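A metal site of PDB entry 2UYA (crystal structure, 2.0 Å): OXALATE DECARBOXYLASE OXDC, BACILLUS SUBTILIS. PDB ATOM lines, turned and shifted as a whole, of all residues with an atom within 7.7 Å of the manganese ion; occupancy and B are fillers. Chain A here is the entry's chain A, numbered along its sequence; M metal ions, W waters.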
ATOM      1  N   MET A  84     -20.014 -24.766  -8.443  1.00  0.00           N
ATOM      2  CA  MET A  84     -19.274 -24.333  -7.264  1.00  0.00           C
ATOM      3  C   MET A  84     -18.796 -25.578  -6.501  1.00  0.00           C
ATOM      4  O   MET A  84     -19.552 -26.554  -6.318  1.00  0.00           O
ATOM      5  CB  MET A  84     -20.122 -23.462  -6.325  1.00  0.00           C
ATOM      6  CG  MET A  84     -19.368 -22.940  -5.084  1.00  0.00           C
ATOM      7  SD  MET A  84     -20.249 -21.643  -4.214  1.00  0.00           S
ATOM      8  CE  MET A  84     -19.883 -20.306  -5.340  1.00  0.00           C
ATOM      9  N   ARG A  92     -19.196 -20.699   1.689  1.00  0.00           N
ATOM     10  CA  ARG A  92     -19.672 -19.660   0.775  1.00  0.00           C
ATOM     11  C   ARG A  92     -20.400 -18.588   1.600  1.00  0.00           C
ATOM     12  O   ARG A  92     -21.455 -18.808   2.198  1.00  0.00           O
ATOM     13  CB  ARG A  92     -20.591 -20.265  -0.310  1.00  0.00           C
ATOM     14  CG  ARG A  92     -21.256 -19.220  -1.251  1.00  0.00           C
ATOM     15  CD  ARG A  92     -20.242 -18.434  -2.049  1.00  0.00           C
ATOM     16  NE  ARG A  92     -20.908 -17.476  -2.958  1.00  0.00           N
ATOM     17  CZ  ARG A  92     -21.086 -16.168  -2.733  1.00  0.00           C
ATOM     18  NH1 ARG A  92     -20.688 -15.596  -1.605  1.00  0.00           N
ATOM     19  NH2 ARG A  92     -21.692 -15.404  -3.645  1.00  0.00           N
ATOM     20  N   GLU A  93     -19.749 -17.443   1.678  1.00  0.00           N
ATOM     21  CA  GLU A  93     -20.087 -16.359   2.552  1.00  0.00           C
ATOM     22  C   GLU A  93     -21.573 -15.977   2.455  1.00  0.00           C
ATOM     23  O   GLU A  93     -22.161 -15.925   1.356  1.00  0.00           O
ATOM     24  CB  GLU A  93     -19.198 -15.137   2.173  1.00  0.00           C
ATOM     25  CG  GLU A  93     -19.558 -13.923   2.930  1.00  0.00           C
ATOM     26  CD  GLU A  93     -18.724 -12.675   2.675  1.00  0.00           C
ATOM     27  OE1 GLU A  93     -17.825 -12.635   1.804  1.00  0.00           O
ATOM     28  OE2 GLU A  93     -19.016 -11.701   3.371  1.00  0.00           O
ATOM     29  N   HIS A  95     -24.745 -14.126   2.012  1.00  0.00           N
ATOM     30  CA  HIS A  95     -24.974 -13.220   0.897  1.00  0.00           C
ATOM     31  C   HIS A  95     -26.438 -13.288   0.426  1.00  0.00           C
ATOM     32  O   HIS A  95     -27.231 -14.145   0.867  1.00  0.00           O
ATOM     33  CB  HIS A  95     -23.999 -13.561  -0.276  1.00  0.00           C
ATOM     34  CG  HIS A  95     -24.340 -14.831  -0.981  1.00  0.00           C
ATOM     35  ND1 HIS A  95     -23.954 -16.081  -0.505  1.00  0.00           N
ATOM     36  CD2 HIS A  95     -25.066 -15.050  -2.099  1.00  0.00           C
ATOM     37  CE1 HIS A  95     -24.442 -17.014  -1.317  1.00  0.00           C
ATOM     38  NE2 HIS A  95     -25.147 -16.416  -2.275  1.00  0.00           N
ATOM     39  N   TRP A  96     -26.780 -12.398  -0.495  1.00  0.00           N
ATOM     40  CA  TRP A  96     -28.073 -12.391  -1.122  1.00  0.00           C
ATOM     41  C   TRP A  96     -27.946 -11.853  -2.551  1.00  0.00           C
ATOM     42  O   TRP A  96     -26.912 -11.327  -2.959  1.00  0.00           O
ATOM     43  CB  TRP A  96     -29.111 -11.593  -0.284  1.00  0.00           C
ATOM     44  CG  TRP A  96     -28.962 -10.068  -0.321  1.00  0.00           C
ATOM     45  CD1 TRP A  96     -29.700  -9.199  -1.065  1.00  0.00           C
ATOM     46  CD2 TRP A  96     -28.052  -9.255   0.444  1.00  0.00           C
ATOM     47  NE1 TRP A  96     -29.302  -7.915  -0.837  1.00  0.00           N
ATOM     48  CE2 TRP A  96     -28.304  -7.910   0.094  1.00  0.00           C
ATOM     49  CE3 TRP A  96     -27.089  -9.528   1.423  1.00  0.00           C
ATOM     50  CZ2 TRP A  96     -27.589  -6.851   0.636  1.00  0.00           C
ATOM     51  CZ3 TRP A  96     -26.358  -8.470   1.932  1.00  0.00           C
ATOM     52  CH2 TRP A  96     -26.617  -7.145   1.544  1.00  0.00           C
ATOM     53  N   HIS A  97     -29.027 -12.016  -3.312  1.00  0.00           N
ATOM     54  CA  HIS A  97     -29.080 -11.436  -4.651  1.00  0.00           C
ATOM     55  C   HIS A  97     -30.525 -11.302  -5.146  1.00  0.00           C
ATOM     56  O   HIS A  97     -31.429 -11.899  -4.578  1.00  0.00           O
ATOM     57  CB  HIS A  97     -28.272 -12.290  -5.651  1.00  0.00           C
ATOM     58  CG  HIS A  97     -28.268 -13.750  -5.331  1.00  0.00           C
ATOM     59  ND1 HIS A  97     -29.393 -14.540  -5.400  1.00  0.00           N
ATOM     60  CD2 HIS A  97     -27.283 -14.542  -4.857  1.00  0.00           C
ATOM     61  CE1 HIS A  97     -29.094 -15.758  -4.989  1.00  0.00           C
ATOM     62  NE2 HIS A  97     -27.822 -15.779  -4.649  1.00  0.00           N
ATOM     63  N   GLU A  99     -31.847 -12.515  -7.888  1.00  0.00           N
ATOM     64  CA  GLU A  99     -32.259 -13.735  -8.498  1.00  0.00           C
ATOM     65  C   GLU A  99     -32.633 -14.778  -7.453  1.00  0.00           C
ATOM     66  O   GLU A  99     -31.989 -14.863  -6.385  1.00  0.00           O
ATOM     67  CB  GLU A  99     -31.111 -14.285  -9.363  1.00  0.00           C
ATOM     68  CG  GLU A  99     -30.659 -13.361 -10.498  1.00  0.00           C
ATOM     69  CD  GLU A  99     -29.609 -12.302 -10.098  1.00  0.00           C
ATOM     70  OE1 GLU A  99     -29.210 -12.169  -8.925  1.00  0.00           O
ATOM     71  OE2 GLU A  99     -29.163 -11.577 -10.986  1.00  0.00           O
ATOM     72  N   ALA A 100     -33.658 -15.562  -7.752  1.00  0.00           N
ATOM     73  CA  ALA A 100     -33.922 -16.824  -7.061  1.00  0.00           C
ATOM     74  C   ALA A 100     -32.829 -17.803  -7.481  1.00  0.00           C
ATOM     75  O   ALA A 100     -32.256 -17.706  -8.576  1.00  0.00           O
ATOM     76  CB  ALA A 100     -35.366 -17.402  -7.424  1.00  0.00           C
ATOM     77  N   GLU A 101     -32.531 -18.727  -6.565  1.00  0.00           N
ATOM     78  CA  GLU A 101     -31.473 -19.686  -6.718  1.00  0.00           C
ATOM     79  C   GLU A 101     -32.020 -21.106  -6.476  1.00  0.00           C
ATOM     80  O   GLU A 101     -32.664 -21.362  -5.473  1.00  0.00           O
ATOM     81  CB  GLU A 101     -30.351 -19.384  -5.746  1.00  0.00           C
ATOM     82  CG  GLU A 101     -29.269 -20.479  -5.639  1.00  0.00           C
ATOM     83  CD  GLU A 101     -28.181 -20.026  -4.671  1.00  0.00           C
ATOM     84  OE1 GLU A 101     -27.900 -18.801  -4.636  1.00  0.00           O
ATOM     85  OE2 GLU A 101     -27.619 -20.867  -3.924  1.00  0.00           O
ATOM     86  N   TRP A 132     -31.838 -27.427  -3.160  1.00  0.00           N
ATOM     87  CA  TRP A 132     -32.365 -26.280  -2.445  1.00  0.00           C
ATOM     88  C   TRP A 132     -32.969 -25.241  -3.409  1.00  0.00           C
ATOM     89  O   TRP A 132     -32.713 -25.276  -4.601  1.00  0.00           O
ATOM     90  CB  TRP A 132     -31.374 -25.649  -1.444  1.00  0.00           C
ATOM     91  CG  TRP A 132     -30.177 -24.927  -1.976  1.00  0.00           C
ATOM     92  CD1 TRP A 132     -30.162 -23.702  -2.610  1.00  0.00           C
ATOM     93  CD2 TRP A 132     -28.809 -25.350  -1.901  1.00  0.00           C
ATOM     94  NE1 TRP A 132     -28.877 -23.360  -2.951  1.00  0.00           N
ATOM     95  CE2 TRP A 132     -28.017 -24.335  -2.498  1.00  0.00           C
ATOM     96  CE3 TRP A 132     -28.163 -26.488  -1.400  1.00  0.00           C
ATOM     97  CZ2 TRP A 132     -26.639 -24.444  -2.628  1.00  0.00           C
ATOM     98  CZ3 TRP A 132     -26.818 -26.582  -1.505  1.00  0.00           C
ATOM     99  CH2 TRP A 132     -26.044 -25.556  -2.096  1.00  0.00           C
ATOM    100  N   PHE A 134     -33.784 -20.933  -2.974  1.00  0.00           N
ATOM    101  CA  PHE A 134     -33.799 -19.731  -2.182  1.00  0.00           C
ATOM    102  C   PHE A 134     -34.545 -18.668  -2.967  1.00  0.00           C
ATOM    103  O   PHE A 134     -34.081 -18.249  -4.031  1.00  0.00           O
ATOM    104  CB  PHE A 134     -32.386 -19.279  -1.863  1.00  0.00           C
ATOM    105  CG  PHE A 134     -31.545 -20.309  -1.102  1.00  0.00           C
ATOM    106  CD1 PHE A 134     -32.123 -21.160  -0.169  1.00  0.00           C
ATOM    107  CD2 PHE A 134     -30.173 -20.373  -1.302  1.00  0.00           C
ATOM    108  CE1 PHE A 134     -31.369 -22.056   0.539  1.00  0.00           C
ATOM    109  CE2 PHE A 134     -29.390 -21.285  -0.577  1.00  0.00           C
ATOM    110  CZ  PHE A 134     -30.013 -22.121   0.323  1.00  0.00           C
ATOM    111  N   LEU A 138     -33.614 -13.374  -0.411  1.00  0.00           N
ATOM    112  CA  LEU A 138     -33.502 -13.920   0.964  1.00  0.00           C
ATOM    113  C   LEU A 138     -32.066 -14.374   1.166  1.00  0.00           C
ATOM    114  O   LEU A 138     -31.482 -14.992   0.274  1.00  0.00           O
ATOM    115  CB  LEU A 138     -34.510 -15.048   1.227  1.00  0.00           C
ATOM    116  CG  LEU A 138     -35.998 -14.679   1.151  1.00  0.00           C
ATOM    117  CD1 LEU A 138     -36.896 -15.858   1.552  1.00  0.00           C
ATOM    118  CD2 LEU A 138     -36.327 -13.389   1.978  1.00  0.00           C
ATOM    119  N   PRO A 139     -31.451 -13.964   2.281  1.00  0.00           N
ATOM    120  CA  PRO A 139     -30.034 -14.167   2.521  1.00  0.00           C
ATOM    121  C   PRO A 139     -29.734 -15.584   2.994  1.00  0.00           C
ATOM    122  O   PRO A 139     -30.502 -16.183   3.762  1.00  0.00           O
ATOM    123  CB  PRO A 139     -29.723 -13.134   3.596  1.00  0.00           C
ATOM    124  CG  PRO A 139     -31.014 -13.024   4.376  1.00  0.00           C
ATOM    125  CD  PRO A 139     -32.102 -13.213   3.378  1.00  0.00           C
ATOM    126  N   HIS A 140     -28.597 -16.090   2.536  1.00  0.00           N
ATOM    127  CA  HIS A 140     -28.262 -17.465   2.723  1.00  0.00           C
ATOM    128  C   HIS A 140     -26.728 -17.690   2.697  1.00  0.00           C
ATOM    129  O   HIS A 140     -25.937 -16.792   2.365  1.00  0.00           O
ATOM    130  CB  HIS A 140     -28.989 -18.325   1.676  1.00  0.00           C
ATOM    131  CG  HIS A 140     -28.744 -17.885   0.262  1.00  0.00           C
ATOM    132  ND1 HIS A 140     -29.537 -16.941  -0.370  1.00  0.00           N
ATOM    133  CD2 HIS A 140     -27.777 -18.210  -0.618  1.00  0.00           C
ATOM    134  CE1 HIS A 140     -29.089 -16.741  -1.595  1.00  0.00           C
ATOM    135  NE2 HIS A 140     -28.023 -17.507  -1.773  1.00  0.00           N
ATOM    136  N   SER A 141     -26.354 -18.888   3.102  1.00  0.00           N
ATOM    137  CA  SER A 141     -24.975 -19.342   3.135  1.00  0.00           C
ATOM    138  C   SER A 141     -24.927 -20.829   2.838  1.00  0.00           C
ATOM    139  O   SER A 141     -25.965 -21.534   2.904  1.00  0.00           O
ATOM    140  CB  SER A 141     -24.358 -19.073   4.500  1.00  0.00           C
ATOM    141  OG  SER A 141     -24.996 -19.917   5.491  1.00  0.00           O
ATOM    142  N   ILE A 142     -23.731 -21.312   2.473  1.00  0.00           N
ATOM    143  CA  ILE A 142     -23.473 -22.723   2.252  1.00  0.00           C
ATOM    144  C   ILE A 142     -22.146 -23.042   2.939  1.00  0.00           C
ATOM    145  O   ILE A 142     -21.201 -22.273   2.796  1.00  0.00           O
ATOM    146  CB  ILE A 142     -23.275 -23.067   0.741  1.00  0.00           C
ATOM    147  CG1 ILE A 142     -24.384 -22.461  -0.138  1.00  0.00           C
ATOM    148  CG2 ILE A 142     -23.218 -24.618   0.535  1.00  0.00           C
ATOM    149  CD1 ILE A 142     -23.956 -22.250  -1.664  1.00  0.00           C
ATOM    150  N   LEU A 153     -25.623 -24.587  -9.360  1.00  0.00           N
ATOM    151  CA  LEU A 153     -26.573 -23.550  -8.994  1.00  0.00           C
ATOM    152  C   LEU A 153     -27.194 -23.026 -10.274  1.00  0.00           C
ATOM    153  O   LEU A 153     -26.496 -22.854 -11.268  1.00  0.00           O
ATOM    154  CB  LEU A 153     -25.847 -22.389  -8.318  1.00  0.00           C
ATOM    155  CG  LEU A 153     -25.104 -22.693  -7.007  1.00  0.00           C
ATOM    156  CD1 LEU A 153     -24.275 -21.511  -6.547  1.00  0.00           C
ATOM    157  CD2 LEU A 153     -26.032 -23.189  -5.925  1.00  0.00           C
ATOM    158  N   PHE A 155     -29.778 -19.796 -11.555  1.00  0.00           N
ATOM    159  CA  PHE A 155     -30.376 -18.515 -11.197  1.00  0.00           C
ATOM    160  C   PHE A 155     -31.364 -18.138 -12.252  1.00  0.00           C
ATOM    161  O   PHE A 155     -31.090 -18.336 -13.435  1.00  0.00           O
ATOM    162  CB  PHE A 155     -29.311 -17.442 -11.108  1.00  0.00           C
ATOM    163  CG  PHE A 155     -28.233 -17.779 -10.142  1.00  0.00           C
ATOM    164  CD1 PHE A 155     -27.071 -18.379 -10.580  1.00  0.00           C
ATOM    165  CD2 PHE A 155     -28.444 -17.614  -8.776  1.00  0.00           C
ATOM    166  CE1 PHE A 155     -26.100 -18.750  -9.697  1.00  0.00           C
ATOM    167  CE2 PHE A 155     -27.464 -17.953  -7.876  1.00  0.00           C
ATOM    168  CZ  PHE A 155     -26.278 -18.522  -8.332  1.00  0.00           C
ATOM    169  N   PHE A 160     -27.100 -12.835 -14.619  1.00  0.00           N
ATOM    170  CA  PHE A 160     -26.431 -13.007 -13.318  1.00  0.00           C
ATOM    171  C   PHE A 160     -24.951 -12.706 -13.348  1.00  0.00           C
ATOM    172  O   PHE A 160     -24.198 -13.304 -14.149  1.00  0.00           O
ATOM    173  CB  PHE A 160     -26.610 -14.477 -12.855  1.00  0.00           C
ATOM    174  CG  PHE A 160     -25.896 -14.804 -11.591  1.00  0.00           C
ATOM    175  CD1 PHE A 160     -26.490 -14.560 -10.362  1.00  0.00           C
ATOM    176  CD2 PHE A 160     -24.623 -15.354 -11.624  1.00  0.00           C
ATOM    177  CE1 PHE A 160     -25.809 -14.865  -9.179  1.00  0.00           C
ATOM    178  CE2 PHE A 160     -23.946 -15.676 -10.443  1.00  0.00           C
ATOM    179  CZ  PHE A 160     -24.550 -15.414  -9.242  1.00  0.00           C
ATOM    180  N   THR A 163     -23.207 -10.744  -6.507  1.00  0.00           N
ATOM    181  CA  THR A 163     -24.049 -11.034  -5.377  1.00  0.00           C
ATOM    182  C   THR A 163     -23.661 -10.018  -4.316  1.00  0.00           C
ATOM    183  O   THR A 163     -22.596  -9.405  -4.390  1.00  0.00           O
ATOM    184  CB  THR A 163     -23.857 -12.509  -4.911  1.00  0.00           C
ATOM    185  OG1 THR A 163     -22.544 -12.682  -4.417  1.00  0.00           O
ATOM    186  CG2 THR A 163     -24.112 -13.489  -6.035  1.00  0.00           C
ATOM    187  N   GLN A 165     -22.552  -9.504  -0.689  1.00  0.00           N
ATOM    188  CA  GLN A 165     -21.851 -10.225   0.399  1.00  0.00           C
ATOM    189  C   GLN A 165     -21.920  -9.388   1.668  1.00  0.00           C
ATOM    190  O   GLN A 165     -21.680  -8.171   1.655  1.00  0.00           O
ATOM    191  CB  GLN A 165     -20.386 -10.412   0.075  1.00  0.00           C
ATOM    192  CG  GLN A 165     -19.982 -11.750  -0.505  1.00  0.00           C
ATOM    193  CD  GLN A 165     -20.418 -11.893  -1.866  1.00  0.00           C
ATOM    194  OE1 GLN A 165     -21.397 -12.603  -2.129  1.00  0.00           O
ATOM    195  NE2 GLN A 165     -19.759 -11.182  -2.790  1.00  0.00           N
HETATM  196 MN    MN M   1     -26.636 -17.505  -3.605  1.00  0.00          MN
HETATM  197  O   HOH W   1     -25.162 -17.245  -5.367  1.00  0.00           O
HETATM  198  O   HOH W   2     -25.574 -19.530  -2.986  1.00  0.00           O
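The backbone carbonyl oxygen (O) of Glu 93 lies within hydrogen-bond range of a ring nitrogen (ND1) of His 95, at 2.6 Å. The side-chain carboxylate (OE2) of Glu 101 lies within hydrogen-bond range of the indole nitrogen (NE1) of Trp 132 (3.0 Å). The backbone NH (N) of Phe 134 is in hydrogen-bond range of the backbone carbonyl oxygen (O) of Glu 101, at 2.8 Å. A ring nitrogen (ND1) of His 97 is in hydrogen-bond range of the backbone carbonyl oxygen of Glu 99. A ring nitrogen (ND1) of His 140 lies within hydrogen-bond range of the backbone carbonyl oxygen (O) of Leu 138, at 2.8 Å. A ring nitrogen (ND1) of His 95 is in hydrogen-bond range of the guanidinium group of Arg 92.
Four residues have an atom within 4 Å of the manganese ion: His 95, His 97, Glu 101 and His 140. The nearest printed residue that does not touch the manganese ion is Phe 155 (4.4 Å).
The manganese ion is bound by OE1 of Glu 101 (2.1 Å), NE2 of His 95 (2.3 Å), NE2 of His 140 (2.3 Å), water W1 (2.3 Å), NE2 of His 97 (2.3 Å) and water W2 (2.4 Å).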
